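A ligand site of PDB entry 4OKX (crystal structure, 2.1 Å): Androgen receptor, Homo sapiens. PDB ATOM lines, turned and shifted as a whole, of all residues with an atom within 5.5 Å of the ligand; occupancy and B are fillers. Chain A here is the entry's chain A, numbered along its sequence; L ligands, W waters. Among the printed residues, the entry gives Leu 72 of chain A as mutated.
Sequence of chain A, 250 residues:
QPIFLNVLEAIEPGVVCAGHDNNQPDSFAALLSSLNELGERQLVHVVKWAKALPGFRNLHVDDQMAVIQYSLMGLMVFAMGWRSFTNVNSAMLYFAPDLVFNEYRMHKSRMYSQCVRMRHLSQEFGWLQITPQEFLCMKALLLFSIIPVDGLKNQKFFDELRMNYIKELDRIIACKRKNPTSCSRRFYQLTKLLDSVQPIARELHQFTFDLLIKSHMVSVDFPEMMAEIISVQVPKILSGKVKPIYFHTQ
Water W2 lies within hydrogen-bond range of O of Gln 69 (2.8 Å), NE2 of His 205 (2.8 Å), N of Met 73 (3.0 Å) and N of Leu 72 (3.3 Å). Water W1 lies within hydrogen-bond range of the backbone carbonyl oxygen (O) of Met 76 (2.8 Å), the guanidinium group (NH2) of Arg 83 (2.8 Å), the side-chain amide nitrogen (NE2) of Gln 42 (3.0 Å) and a nitrogen (N2) of the ligand (3.2 Å).
The side-chain amide nitrogen of Asn 36 sits close to the backbone carbonyl oxygen of Leu 32 (3.2 Å). The guanidinium group (NH2) of Arg 83 sits at hydrogen-bond distance from the side-chain amide oxygen (OE1) of Gln 42 (3.4 Å). The guanidinium group of Arg 83 sits at hydrogen-bond distance from the backbone carbonyl oxygen of Phe 95. The guanidinium group (NE) of Arg 83 is in hydrogen-bond range of the backbone carbonyl oxygen (O) of Tyr 94 (3.2 Å). SD of Met 76 lies close to NE2 of Gln 42. The side-chain hydroxyl (OG1) of Thr 208 is in hydrogen-bond range of the backbone carbonyl oxygen (O) of Leu 204, at 2.8 Å. N of Val 234 lies within hydrogen-bond range of O of Ile 229, at 3.2 Å.
The backbone NH of Asn 36 sits close to an oxygen (O3) of the ligand, at 3.2 Å. An oxygen (O3) of the ligand lies within hydrogen-bond range of the side-chain amide oxygen (OD1) of Asn 36 (2.5 Å). The guanidinium group of Arg 83 lies within hydrogen-bond range of a nitrogen (N2) of the ligand (2.9 Å). The backbone carbonyl oxygen (O) of Leu 35 sits at hydrogen-bond distance from an oxygen (O3) of the ligand (3.1 Å). A nitrogen (N2) of the ligand lies close to the side-chain amide oxygen of Gln 42, 3.5 Å away.
O4 of the ligand sits close to SD of Met 73, at 3.5 Å. F2 of the ligand lies close to N of Val 77, at 3.3 Å. The side-chain sulfur of Met 118 lies close to a fluorine (F4) of the ligand (3.7 Å). Residues that only touch the ligand: Gly 39 (3.4 Å), Met 80 (3.4 Å), Met 76 (3.4 Å), Thr 208 (3.5 Å), His 205 (3.5 Å), Phe 95 (3.6 Å), Leu 204 (3.7 Å), Val 234 (3.7 Å), Met 226 (3.7 Å), Ile 230 (3.7 Å), Leu 72 (3.8 Å), Leu 38 (3.8 Å) and Gln 69 (3.9 Å). Of the 29 residues printed, 20 come within 4 Å of the ligand.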
ATOM      1  N   LEU A  32     -29.187 -25.086  23.235  1.00  0.00           N
ATOM      2  CA  LEU A  32     -28.209 -24.462  22.375  1.00  0.00           C
ATOM      3  C   LEU A  32     -27.096 -25.392  21.912  1.00  0.00           C
ATOM      4  O   LEU A  32     -26.591 -25.198  20.834  1.00  0.00           O
ATOM      5  CB  LEU A  32     -27.645 -23.247  23.031  1.00  0.00           C
ATOM      6  CG  LEU A  32     -28.595 -22.093  22.805  1.00  0.00           C
ATOM      7  CD1 LEU A  32     -28.145 -21.090  23.798  1.00  0.00           C
ATOM      8  CD2 LEU A  32     -28.546 -21.525  21.389  1.00  0.00           C
ATOM      9  N   LEU A  35     -28.700 -27.003  19.062  1.00  0.00           N
ATOM     10  CA  LEU A  35     -28.771 -26.068  17.955  1.00  0.00           C
ATOM     11  C   LEU A  35     -27.427 -25.897  17.226  1.00  0.00           C
ATOM     12  O   LEU A  35     -27.378 -25.759  16.020  1.00  0.00           O
ATOM     13  CB  LEU A  35     -29.367 -24.704  18.386  1.00  0.00           C
ATOM     14  CG  LEU A  35     -30.922 -24.528  18.383  1.00  0.00           C
ATOM     15  CD1 LEU A  35     -31.407 -23.180  18.880  1.00  0.00           C
ATOM     16  CD2 LEU A  35     -31.501 -24.667  16.981  1.00  0.00           C
ATOM     17  N   ASN A  36     -26.353 -25.850  18.001  1.00  0.00           N
ATOM     18  CA  ASN A  36     -24.993 -25.732  17.463  1.00  0.00           C
ATOM     19  C   ASN A  36     -24.627 -26.998  16.707  1.00  0.00           C
ATOM     20  O   ASN A  36     -24.034 -26.941  15.643  1.00  0.00           O
ATOM     21  CB  ASN A  36     -23.999 -25.518  18.599  1.00  0.00           C
ATOM     22  CG  ASN A  36     -24.160 -24.201  19.309  1.00  0.00           C
ATOM     23  OD1 ASN A  36     -24.702 -23.225  18.768  1.00  0.00           O
ATOM     24  ND2 ASN A  36     -23.603 -24.130  20.481  1.00  0.00           N
ATOM     25  N   GLU A  37     -24.987 -28.137  17.249  1.00  0.00           N
ATOM     26  CA  GLU A  37     -24.754 -29.395  16.517  1.00  0.00           C
ATOM     27  C   GLU A  37     -25.554 -29.444  15.218  1.00  0.00           C
ATOM     28  O   GLU A  37     -25.038 -29.876  14.177  1.00  0.00           O
ATOM     29  CB  GLU A  37     -25.050 -30.607  17.415  1.00  0.00           C
ATOM     30  CG  GLU A  37     -25.022 -31.965  16.743  1.00  0.00           C
ATOM     31  CD  GLU A  37     -23.649 -32.320  16.171  1.00  0.00           C
ATOM     32  OE1 GLU A  37     -23.583 -33.144  15.236  1.00  0.00           O
ATOM     33  OE2 GLU A  37     -22.628 -31.787  16.627  1.00  0.00           O
ATOM     34  N   LEU A  38     -26.821 -29.026  15.276  1.00  0.00           N
ATOM     35  CA  LEU A  38     -27.671 -29.019  14.076  1.00  0.00           C
ATOM     36  C   LEU A  38     -27.108 -28.077  13.062  1.00  0.00           C
ATOM     37  O   LEU A  38     -27.133 -28.372  11.868  1.00  0.00           O
ATOM     38  CB  LEU A  38     -29.125 -28.612  14.433  1.00  0.00           C
ATOM     39  CG  LEU A  38     -30.106 -28.588  13.261  1.00  0.00           C
ATOM     40  CD1 LEU A  38     -30.244 -29.942  12.543  1.00  0.00           C
ATOM     41  CD2 LEU A  38     -31.438 -28.159  13.820  1.00  0.00           C
ATOM     42  N   GLY A  39     -26.532 -26.955  13.543  1.00  0.00           N
ATOM     43  CA  GLY A  39     -25.936 -25.994  12.647  1.00  0.00           C
ATOM     44  C   GLY A  39     -24.816 -26.632  11.830  1.00  0.00           C
ATOM     45  O   GLY A  39     -24.734 -26.412  10.636  1.00  0.00           O
ATOM     46  N   GLU A  40     -23.966 -27.447  12.448  1.00  0.00           N
ATOM     47  CA  GLU A  40     -22.881 -28.107  11.728  1.00  0.00           C
ATOM     48  C   GLU A  40     -23.392 -29.129  10.732  1.00  0.00           C
ATOM     49  O   GLU A  40     -22.861 -29.271   9.670  1.00  0.00           O
ATOM     50  CB  GLU A  40     -21.970 -28.896  12.654  1.00  0.00           C
ATOM     51  CG  GLU A  40     -20.704 -29.320  11.921  1.00  0.00           C
ATOM     52  CD  GLU A  40     -19.676 -29.845  12.893  1.00  0.00           C
ATOM     53  OE1 GLU A  40     -18.571 -29.289  12.935  1.00  0.00           O
ATOM     54  OE2 GLU A  40     -20.022 -30.783  13.643  1.00  0.00           O
ATOM     55  N   GLN A  42     -26.361 -29.117   9.340  1.00  0.00           N
ATOM     56  CA  GLN A  42     -26.902 -28.373   8.192  1.00  0.00           C
ATOM     57  C   GLN A  42     -25.834 -27.729   7.303  1.00  0.00           C
ATOM     58  O   GLN A  42     -25.986 -27.703   6.102  1.00  0.00           O
ATOM     59  CB  GLN A  42     -27.963 -27.329   8.616  1.00  0.00           C
ATOM     60  CG  GLN A  42     -29.226 -28.014   9.166  1.00  0.00           C
ATOM     61  CD  GLN A  42     -30.397 -27.113   9.446  1.00  0.00           C
ATOM     62  OE1 GLN A  42     -31.452 -27.564   9.975  1.00  0.00           O
ATOM     63  NE2 GLN A  42     -30.279 -25.859   9.085  1.00  0.00           N
ATOM     64  N   GLN A  69     -20.151 -19.528   3.860  1.00  0.00           N
ATOM     65  CA  GLN A  69     -20.057 -19.165   5.265  1.00  0.00           C
ATOM     66  C   GLN A  69     -20.839 -17.897   5.639  1.00  0.00           C
ATOM     67  O   GLN A  69     -21.489 -17.866   6.674  1.00  0.00           O
ATOM     68  CB  GLN A  69     -18.591 -19.073   5.702  1.00  0.00           C
ATOM     69  CG  GLN A  69     -17.848 -20.377   5.498  1.00  0.00           C
ATOM     70  CD  GLN A  69     -16.364 -20.150   5.619  1.00  0.00           C
ATOM     71  OE1 GLN A  69     -15.694 -19.741   4.669  1.00  0.00           O
ATOM     72  NE2 GLN A  69     -15.872 -20.336   6.803  1.00  0.00           N
ATOM     73  N   LEU A  72     -24.822 -18.723   5.382  1.00  0.00           N
ATOM     74  CA  LEU A  72     -25.298 -19.950   6.022  1.00  0.00           C
ATOM     75  C   LEU A  72     -26.489 -19.668   6.974  1.00  0.00           C
ATOM     76  O   LEU A  72     -27.464 -20.385   6.928  1.00  0.00           O
ATOM     77  CB  LEU A  72     -24.213 -20.656   6.852  1.00  0.00           C
ATOM     78  CG  LEU A  72     -24.678 -21.826   7.706  1.00  0.00           C
ATOM     79  CD1 LEU A  72     -25.120 -23.008   6.835  1.00  0.00           C
ATOM     80  CD2 LEU A  72     -23.632 -22.321   8.681  1.00  0.00           C
ATOM     81  N   MET A  73     -26.350 -18.695   7.885  1.00  0.00           N
ATOM     82  CA  MET A  73     -27.475 -18.342   8.817  1.00  0.00           C
ATOM     83  C   MET A  73     -28.813 -18.110   8.110  1.00  0.00           C
ATOM     84  O   MET A  73     -29.842 -18.713   8.489  1.00  0.00           O
ATOM     85  CB  MET A  73     -27.136 -17.163   9.715  1.00  0.00           C
ATOM     86  CG  MET A  73     -28.108 -17.001  10.904  1.00  0.00           C
ATOM     87  SD  MET A  73     -28.042 -18.387  12.041  1.00  0.00           S
ATOM     88  CE  MET A  73     -26.614 -17.913  12.980  1.00  0.00           C
ATOM     89  N   MET A  76     -30.365 -21.096   6.473  1.00  0.00           N
ATOM     90  CA  MET A  76     -30.954 -21.981   7.455  1.00  0.00           C
ATOM     91  C   MET A  76     -32.284 -21.413   8.031  1.00  0.00           C
ATOM     92  O   MET A  76     -33.213 -22.176   8.258  1.00  0.00           O
ATOM     93  CB  MET A  76     -29.990 -22.274   8.602  1.00  0.00           C
ATOM     94  CG  MET A  76     -28.769 -23.180   8.291  1.00  0.00           C
ATOM     95  SD  MET A  76     -27.910 -23.645   9.858  1.00  0.00           S
ATOM     96  CE  MET A  76     -27.714 -22.124  10.759  1.00  0.00           C
ATOM     97  N   VAL A  77     -32.346 -20.076   8.185  1.00  0.00           N
ATOM     98  CA  VAL A  77     -33.509 -19.433   8.644  1.00  0.00           C
ATOM     99  C   VAL A  77     -34.596 -19.578   7.660  1.00  0.00           C
ATOM    100  O   VAL A  77     -35.694 -19.921   8.073  1.00  0.00           O
ATOM    101  CB  VAL A  77     -33.251 -17.953   8.930  1.00  0.00           C
ATOM    102  CG1 VAL A  77     -34.541 -17.190   9.116  1.00  0.00           C
ATOM    103  CG2 VAL A  77     -32.326 -17.812  10.141  1.00  0.00           C
ATOM    104  N   MET A  80     -35.807 -23.106   7.375  1.00  0.00           N
ATOM    105  CA  MET A  80     -36.502 -23.517   8.564  1.00  0.00           C
ATOM    106  C   MET A  80     -37.915 -22.944   8.571  1.00  0.00           C
ATOM    107  O   MET A  80     -38.867 -23.653   8.943  1.00  0.00           O
ATOM    108  CB  MET A  80     -35.750 -23.138   9.812  1.00  0.00           C
ATOM    109  CG  MET A  80     -36.327 -23.685  11.108  1.00  0.00           C
ATOM    110  SD  MET A  80     -37.641 -22.637  11.801  1.00  0.00           S
ATOM    111  CE  MET A  80     -36.697 -21.207  12.344  1.00  0.00           C
ATOM    112  N   ARG A  83     -39.964 -25.183   6.341  1.00  0.00           N
ATOM    113  CA  ARG A  83     -40.299 -26.421   7.046  1.00  0.00           C
ATOM    114  C   ARG A  83     -41.407 -26.234   8.044  1.00  0.00           C
ATOM    115  O   ARG A  83     -42.235 -27.116   8.222  1.00  0.00           O
ATOM    116  CB  ARG A  83     -39.103 -26.965   7.854  1.00  0.00           C
ATOM    117  CG  ARG A  83     -38.078 -27.662   6.999  1.00  0.00           C
ATOM    118  CD  ARG A  83     -37.117 -28.504   7.856  1.00  0.00           C
ATOM    119  NE  ARG A  83     -36.343 -27.749   8.803  1.00  0.00           N
ATOM    120  CZ  ARG A  83     -35.289 -27.010   8.471  1.00  0.00           C
ATOM    121  NH1 ARG A  83     -34.904 -26.868   7.231  1.00  0.00           N
ATOM    122  NH2 ARG A  83     -34.631 -26.383   9.413  1.00  0.00           N
ATOM    123  N   TYR A  94     -39.941 -25.535  13.435  1.00  0.00           N
ATOM    124  CA  TYR A  94     -39.469 -26.860  13.103  1.00  0.00           C
ATOM    125  C   TYR A  94     -37.939 -26.840  12.774  1.00  0.00           C
ATOM    126  O   TYR A  94     -37.550 -26.955  11.642  1.00  0.00           O
ATOM    127  CB  TYR A  94     -40.263 -27.383  11.915  1.00  0.00           C
ATOM    128  CG  TYR A  94     -40.324 -28.856  11.786  1.00  0.00           C
ATOM    129  CD1 TYR A  94     -41.385 -29.565  12.306  1.00  0.00           C
ATOM    130  CD2 TYR A  94     -39.373 -29.561  11.076  1.00  0.00           C
ATOM    131  CE1 TYR A  94     -41.491 -30.939  12.164  1.00  0.00           C
ATOM    132  CE2 TYR A  94     -39.465 -30.932  10.906  1.00  0.00           C
ATOM    133  CZ  TYR A  94     -40.512 -31.610  11.465  1.00  0.00           C
ATOM    134  OH  TYR A  94     -40.580 -32.947  11.345  1.00  0.00           O
ATOM    135  N   PHE A  95     -37.090 -26.713  13.753  1.00  0.00           N
ATOM    136  CA  PHE A  95     -35.674 -26.702  13.412  1.00  0.00           C
ATOM    137  C   PHE A  95     -35.305 -28.082  12.794  1.00  0.00           C
ATOM    138  O   PHE A  95     -34.565 -28.172  11.841  1.00  0.00           O
ATOM    139  CB  PHE A  95     -34.838 -26.371  14.605  1.00  0.00           C
ATOM    140  CG  PHE A  95     -34.961 -24.948  15.084  1.00  0.00           C
ATOM    141  CD1 PHE A  95     -34.131 -23.954  14.593  1.00  0.00           C
ATOM    142  CD2 PHE A  95     -35.882 -24.627  16.051  1.00  0.00           C
ATOM    143  CE1 PHE A  95     -34.247 -22.650  15.059  1.00  0.00           C
ATOM    144  CE2 PHE A  95     -36.032 -23.314  16.466  1.00  0.00           C
ATOM    145  CZ  PHE A  95     -35.178 -22.336  15.987  1.00  0.00           C
ATOM    146  N   MET A 111     -33.851 -16.721  22.934  1.00  0.00           N
ATOM    147  CA  MET A 111     -33.899 -16.198  21.584  1.00  0.00           C
ATOM    148  C   MET A 111     -35.314 -15.931  21.190  1.00  0.00           C
ATOM    149  O   MET A 111     -35.705 -16.125  20.019  1.00  0.00           O
ATOM    150  CB  MET A 111     -33.344 -17.233  20.574  1.00  0.00           C
ATOM    151  CG  MET A 111     -32.190 -18.145  21.014  1.00  0.00           C
ATOM    152  SD  MET A 111     -31.800 -19.343  19.682  1.00  0.00           S
ATOM    153  CE  MET A 111     -31.292 -18.078  18.540  1.00  0.00           C
ATOM    154  N   MET A 118     -38.980 -15.337  13.247  1.00  0.00           N
ATOM    155  CA  MET A 118     -38.899 -16.500  12.318  1.00  0.00           C
ATOM    156  C   MET A 118     -40.260 -17.126  12.054  1.00  0.00           C
ATOM    157  O   MET A 118     -40.534 -17.475  10.911  1.00  0.00           O
ATOM    158  CB  MET A 118     -37.881 -17.522  12.843  1.00  0.00           C
ATOM    159  CG  MET A 118     -36.452 -16.992  12.811  1.00  0.00           C
ATOM    160  SD  MET A 118     -35.154 -18.212  13.184  1.00  0.00           S
ATOM    161  CE  MET A 118     -35.162 -18.145  14.949  1.00  0.00           C
ATOM    162  N   LEU A 204     -29.297 -13.180  14.806  1.00  0.00           N
ATOM    163  CA  LEU A 204     -28.810 -14.534  15.155  1.00  0.00           C
ATOM    164  C   LEU A 204     -27.313 -14.586  15.202  1.00  0.00           C
ATOM    165  O   LEU A 204     -26.680 -15.179  16.088  1.00  0.00           O
ATOM    166  CB  LEU A 204     -29.406 -15.556  14.229  1.00  0.00           C
ATOM    167  CG  LEU A 204     -30.885 -15.852  14.570  1.00  0.00           C
ATOM    168  CD1 LEU A 204     -31.556 -16.784  13.547  1.00  0.00           C
ATOM    169  CD2 LEU A 204     -31.060 -16.436  15.987  1.00  0.00           C
ATOM    170  N   HIS A 205     -26.716 -13.948  14.226  1.00  0.00           N
ATOM    171  CA  HIS A 205     -25.298 -13.807  14.211  1.00  0.00           C
ATOM    172  C   HIS A 205     -24.800 -13.162  15.487  1.00  0.00           C
ATOM    173  O   HIS A 205     -23.851 -13.662  16.123  1.00  0.00           O
ATOM    174  CB  HIS A 205     -24.875 -12.971  12.978  1.00  0.00           C
ATOM    175  CG  HIS A 205     -24.689 -13.791  11.745  1.00  0.00           C
ATOM    176  ND1 HIS A 205     -25.000 -13.306  10.496  1.00  0.00           N
ATOM    177  CD2 HIS A 205     -24.221 -15.048  11.566  1.00  0.00           C
ATOM    178  CE1 HIS A 205     -24.707 -14.231   9.595  1.00  0.00           C
ATOM    179  NE2 HIS A 205     -24.232 -15.296  10.216  1.00  0.00           N
ATOM    180  N   PHE A 207     -26.247 -12.813  18.407  1.00  0.00           N
ATOM    181  CA  PHE A 207     -26.523 -13.722  19.527  1.00  0.00           C
ATOM    182  C   PHE A 207     -25.548 -14.860  19.562  1.00  0.00           C
ATOM    183  O   PHE A 207     -24.996 -15.209  20.617  1.00  0.00           O
ATOM    184  CB  PHE A 207     -27.981 -14.227  19.465  1.00  0.00           C
ATOM    185  CG  PHE A 207     -28.286 -15.357  20.411  1.00  0.00           C
ATOM    186  CD1 PHE A 207     -27.959 -16.651  20.076  1.00  0.00           C
ATOM    187  CD2 PHE A 207     -28.928 -15.117  21.625  1.00  0.00           C
ATOM    188  CE1 PHE A 207     -28.244 -17.700  20.955  1.00  0.00           C
ATOM    189  CE2 PHE A 207     -29.222 -16.160  22.500  1.00  0.00           C
ATOM    190  CZ  PHE A 207     -28.873 -17.461  22.166  1.00  0.00           C
ATOM    191  N   THR A 208     -25.261 -15.427  18.396  1.00  0.00           N
ATOM    192  CA  THR A 208     -24.329 -16.604  18.310  1.00  0.00           C
ATOM    193  C   THR A 208     -22.911 -16.231  18.657  1.00  0.00           C
ATOM    194  O   THR A 208     -22.149 -17.009  19.293  1.00  0.00           O
ATOM    195  CB  THR A 208     -24.295 -17.167  16.852  1.00  0.00           C
ATOM    196  OG1 THR A 208     -25.572 -17.730  16.520  1.00  0.00           O
ATOM    197  CG2 THR A 208     -23.215 -18.188  16.686  1.00  0.00           C
ATOM    198  N   LEU A 211     -22.723 -15.547  22.486  1.00  0.00           N
ATOM    199  CA  LEU A 211     -22.782 -16.864  23.122  1.00  0.00           C
ATOM    200  C   LEU A 211     -21.506 -17.622  23.023  1.00  0.00           C
ATOM    201  O   LEU A 211     -21.097 -18.260  23.971  1.00  0.00           O
ATOM    202  CB  LEU A 211     -23.923 -17.670  22.530  1.00  0.00           C
ATOM    203  CG  LEU A 211     -24.058 -19.077  23.074  1.00  0.00           C
ATOM    204  CD1 LEU A 211     -24.229 -18.952  24.562  1.00  0.00           C
ATOM    205  CD2 LEU A 211     -25.257 -19.778  22.395  1.00  0.00           C
ATOM    206  N   PHE A 222     -19.972 -25.812  21.437  1.00  0.00           N
ATOM    207  CA  PHE A 222     -19.861 -25.562  19.980  1.00  0.00           C
ATOM    208  C   PHE A 222     -18.972 -26.516  19.287  1.00  0.00           C
ATOM    209  O   PHE A 222     -17.873 -26.666  19.695  1.00  0.00           O
ATOM    210  CB  PHE A 222     -19.250 -24.230  19.650  1.00  0.00           C
ATOM    211  CG  PHE A 222     -20.140 -23.113  19.890  1.00  0.00           C
ATOM    212  CD1 PHE A 222     -20.192 -22.566  21.149  1.00  0.00           C
ATOM    213  CD2 PHE A 222     -20.982 -22.667  18.903  1.00  0.00           C
ATOM    214  CE1 PHE A 222     -21.047 -21.539  21.413  1.00  0.00           C
ATOM    215  CE2 PHE A 222     -21.847 -21.626  19.151  1.00  0.00           C
ATOM    216  CZ  PHE A 222     -21.882 -21.056  20.407  1.00  0.00           C
ATOM    217  N   MET A 226     -17.771 -24.854  13.650  1.00  0.00           N
ATOM    218  CA  MET A 226     -18.691 -23.761  13.813  1.00  0.00           C
ATOM    219  C   MET A 226     -18.008 -22.664  14.654  1.00  0.00           C
ATOM    220  O   MET A 226     -18.249 -21.475  14.401  1.00  0.00           O
ATOM    221  CB  MET A 226     -19.965 -24.226  14.464  1.00  0.00           C
ATOM    222  CG  MET A 226     -20.633 -25.413  13.740  1.00  0.00           C
ATOM    223  SD  MET A 226     -20.620 -25.254  11.941  1.00  0.00           S
ATOM    224  CE  MET A 226     -22.020 -24.124  11.854  1.00  0.00           C
ATOM    225  N   ILE A 229     -15.770 -20.761  12.268  1.00  0.00           N
ATOM    226  CA  ILE A 229     -16.588 -19.922  11.481  1.00  0.00           C
ATOM    227  C   ILE A 229     -17.054 -18.741  12.306  1.00  0.00           C
ATOM    228  O   ILE A 229     -17.015 -17.584  11.848  1.00  0.00           O
ATOM    229  CB  ILE A 229     -17.799 -20.680  10.886  1.00  0.00           C
ATOM    230  CG1 ILE A 229     -17.328 -21.769   9.878  1.00  0.00           C
ATOM    231  CG2 ILE A 229     -18.760 -19.707  10.231  1.00  0.00           C
ATOM    232  CD1 ILE A 229     -18.417 -22.730   9.428  1.00  0.00           C
ATOM    233  N   ILE A 230     -17.512 -18.990  13.531  1.00  0.00           N
ATOM    234  CA  ILE A 230     -18.006 -17.925  14.317  1.00  0.00           C
ATOM    235  C   ILE A 230     -16.904 -16.921  14.634  1.00  0.00           C
ATOM    236  O   ILE A 230     -17.169 -15.756  14.667  1.00  0.00           O
ATOM    237  CB  ILE A 230     -18.753 -18.385  15.578  1.00  0.00           C
ATOM    238  CG1 ILE A 230     -19.916 -19.311  15.196  1.00  0.00           C
ATOM    239  CG2 ILE A 230     -19.346 -17.161  16.324  1.00  0.00           C
ATOM    240  CD1 ILE A 230     -20.303 -20.284  16.306  1.00  0.00           C
ATOM    241  N   VAL A 234     -17.927 -14.603  11.061  1.00  0.00           N
ATOM    242  CA  VAL A 234     -19.094 -13.845  11.573  1.00  0.00           C
ATOM    243  C   VAL A 234     -18.714 -12.371  11.994  1.00  0.00           C
ATOM    244  O   VAL A 234     -19.528 -11.456  11.783  1.00  0.00           O
ATOM    245  CB  VAL A 234     -19.786 -14.649  12.691  1.00  0.00           C
ATOM    246  CG1 VAL A 234     -20.946 -13.894  13.345  1.00  0.00           C
ATOM    247  CG2 VAL A 234     -20.348 -15.951  12.103  1.00  0.00           C
HETATM  248  C1  LIG L   1     -24.942 -20.592  12.247  1.00  0.00           C
HETATM  249  C2  LIG L   1     -24.476 -19.711  11.250  1.00  0.00           C
HETATM  250  C3  LIG L   1     -23.160 -19.233  11.281  1.00  0.00           C
HETATM  251  F1  LIG L   1     -22.556 -18.387  10.402  1.00  0.00           F
HETATM  252  C4  LIG L   1     -22.318 -19.724  12.261  1.00  0.00           C
HETATM  253  C5  LIG L   1     -22.797 -20.603  13.208  1.00  0.00           C
HETATM  254  C6  LIG L   1     -24.076 -21.082  13.233  1.00  0.00           C
HETATM  255  S1  LIG L   1     -24.460 -22.093  14.449  1.00  0.00           S
HETATM  256  O1  LIG L   1     -25.479 -22.942  13.973  1.00  0.00           O
HETATM  257  O2  LIG L   1     -23.308 -22.715  15.032  1.00  0.00           O
HETATM  258  C7  LIG L   1     -25.083 -21.072  15.714  1.00  0.00           C
HETATM  259  C8  LIG L   1     -26.396 -21.573  16.343  1.00  0.00           C
HETATM  260  O3  LIG L   1     -26.234 -22.953  16.752  1.00  0.00           O
HETATM  261  C9  LIG L   1     -26.886 -20.819  17.593  1.00  0.00           C
HETATM  262  C10 LIG L   1     -27.527 -21.517  15.343  1.00  0.00           C
HETATM  263  O4  LIG L   1     -27.916 -20.478  14.830  1.00  0.00           O
HETATM  264  N1  LIG L   1     -28.059 -22.741  15.090  1.00  0.00           N
HETATM  265  C11 LIG L   1     -29.124 -22.981  14.281  1.00  0.00           C
HETATM  266  C12 LIG L   1     -29.957 -22.013  13.725  1.00  0.00           C
HETATM  267  C13 LIG L   1     -29.293 -24.304  13.883  1.00  0.00           C
HETATM  268  C14 LIG L   1     -30.250 -24.693  12.975  1.00  0.00           C
HETATM  269  C15 LIG L   1     -31.105 -23.780  12.415  1.00  0.00           C
HETATM  270  C16 LIG L   1     -32.033 -24.227  11.664  1.00  0.00           C
HETATM  271  N2  LIG L   1     -32.933 -24.605  10.998  1.00  0.00           N
HETATM  272  C17 LIG L   1     -30.969 -22.364  12.820  1.00  0.00           C
HETATM  273  C18 LIG L   1     -31.872 -21.266  12.287  1.00  0.00           C
HETATM  274  F2  LIG L   1     -31.406 -20.660  11.248  1.00  0.00           F
HETATM  275  F3  LIG L   1     -32.993 -21.724  11.818  1.00  0.00           F
HETATM  276  F4  LIG L   1     -32.134 -20.390  13.244  1.00  0.00           F
HETATM  277  O   HOH W   1     -32.839 -24.905   7.858  1.00  0.00           O
HETATM  278  O   HOH W   2     -23.835 -17.168   8.115  1.00  0.00           O
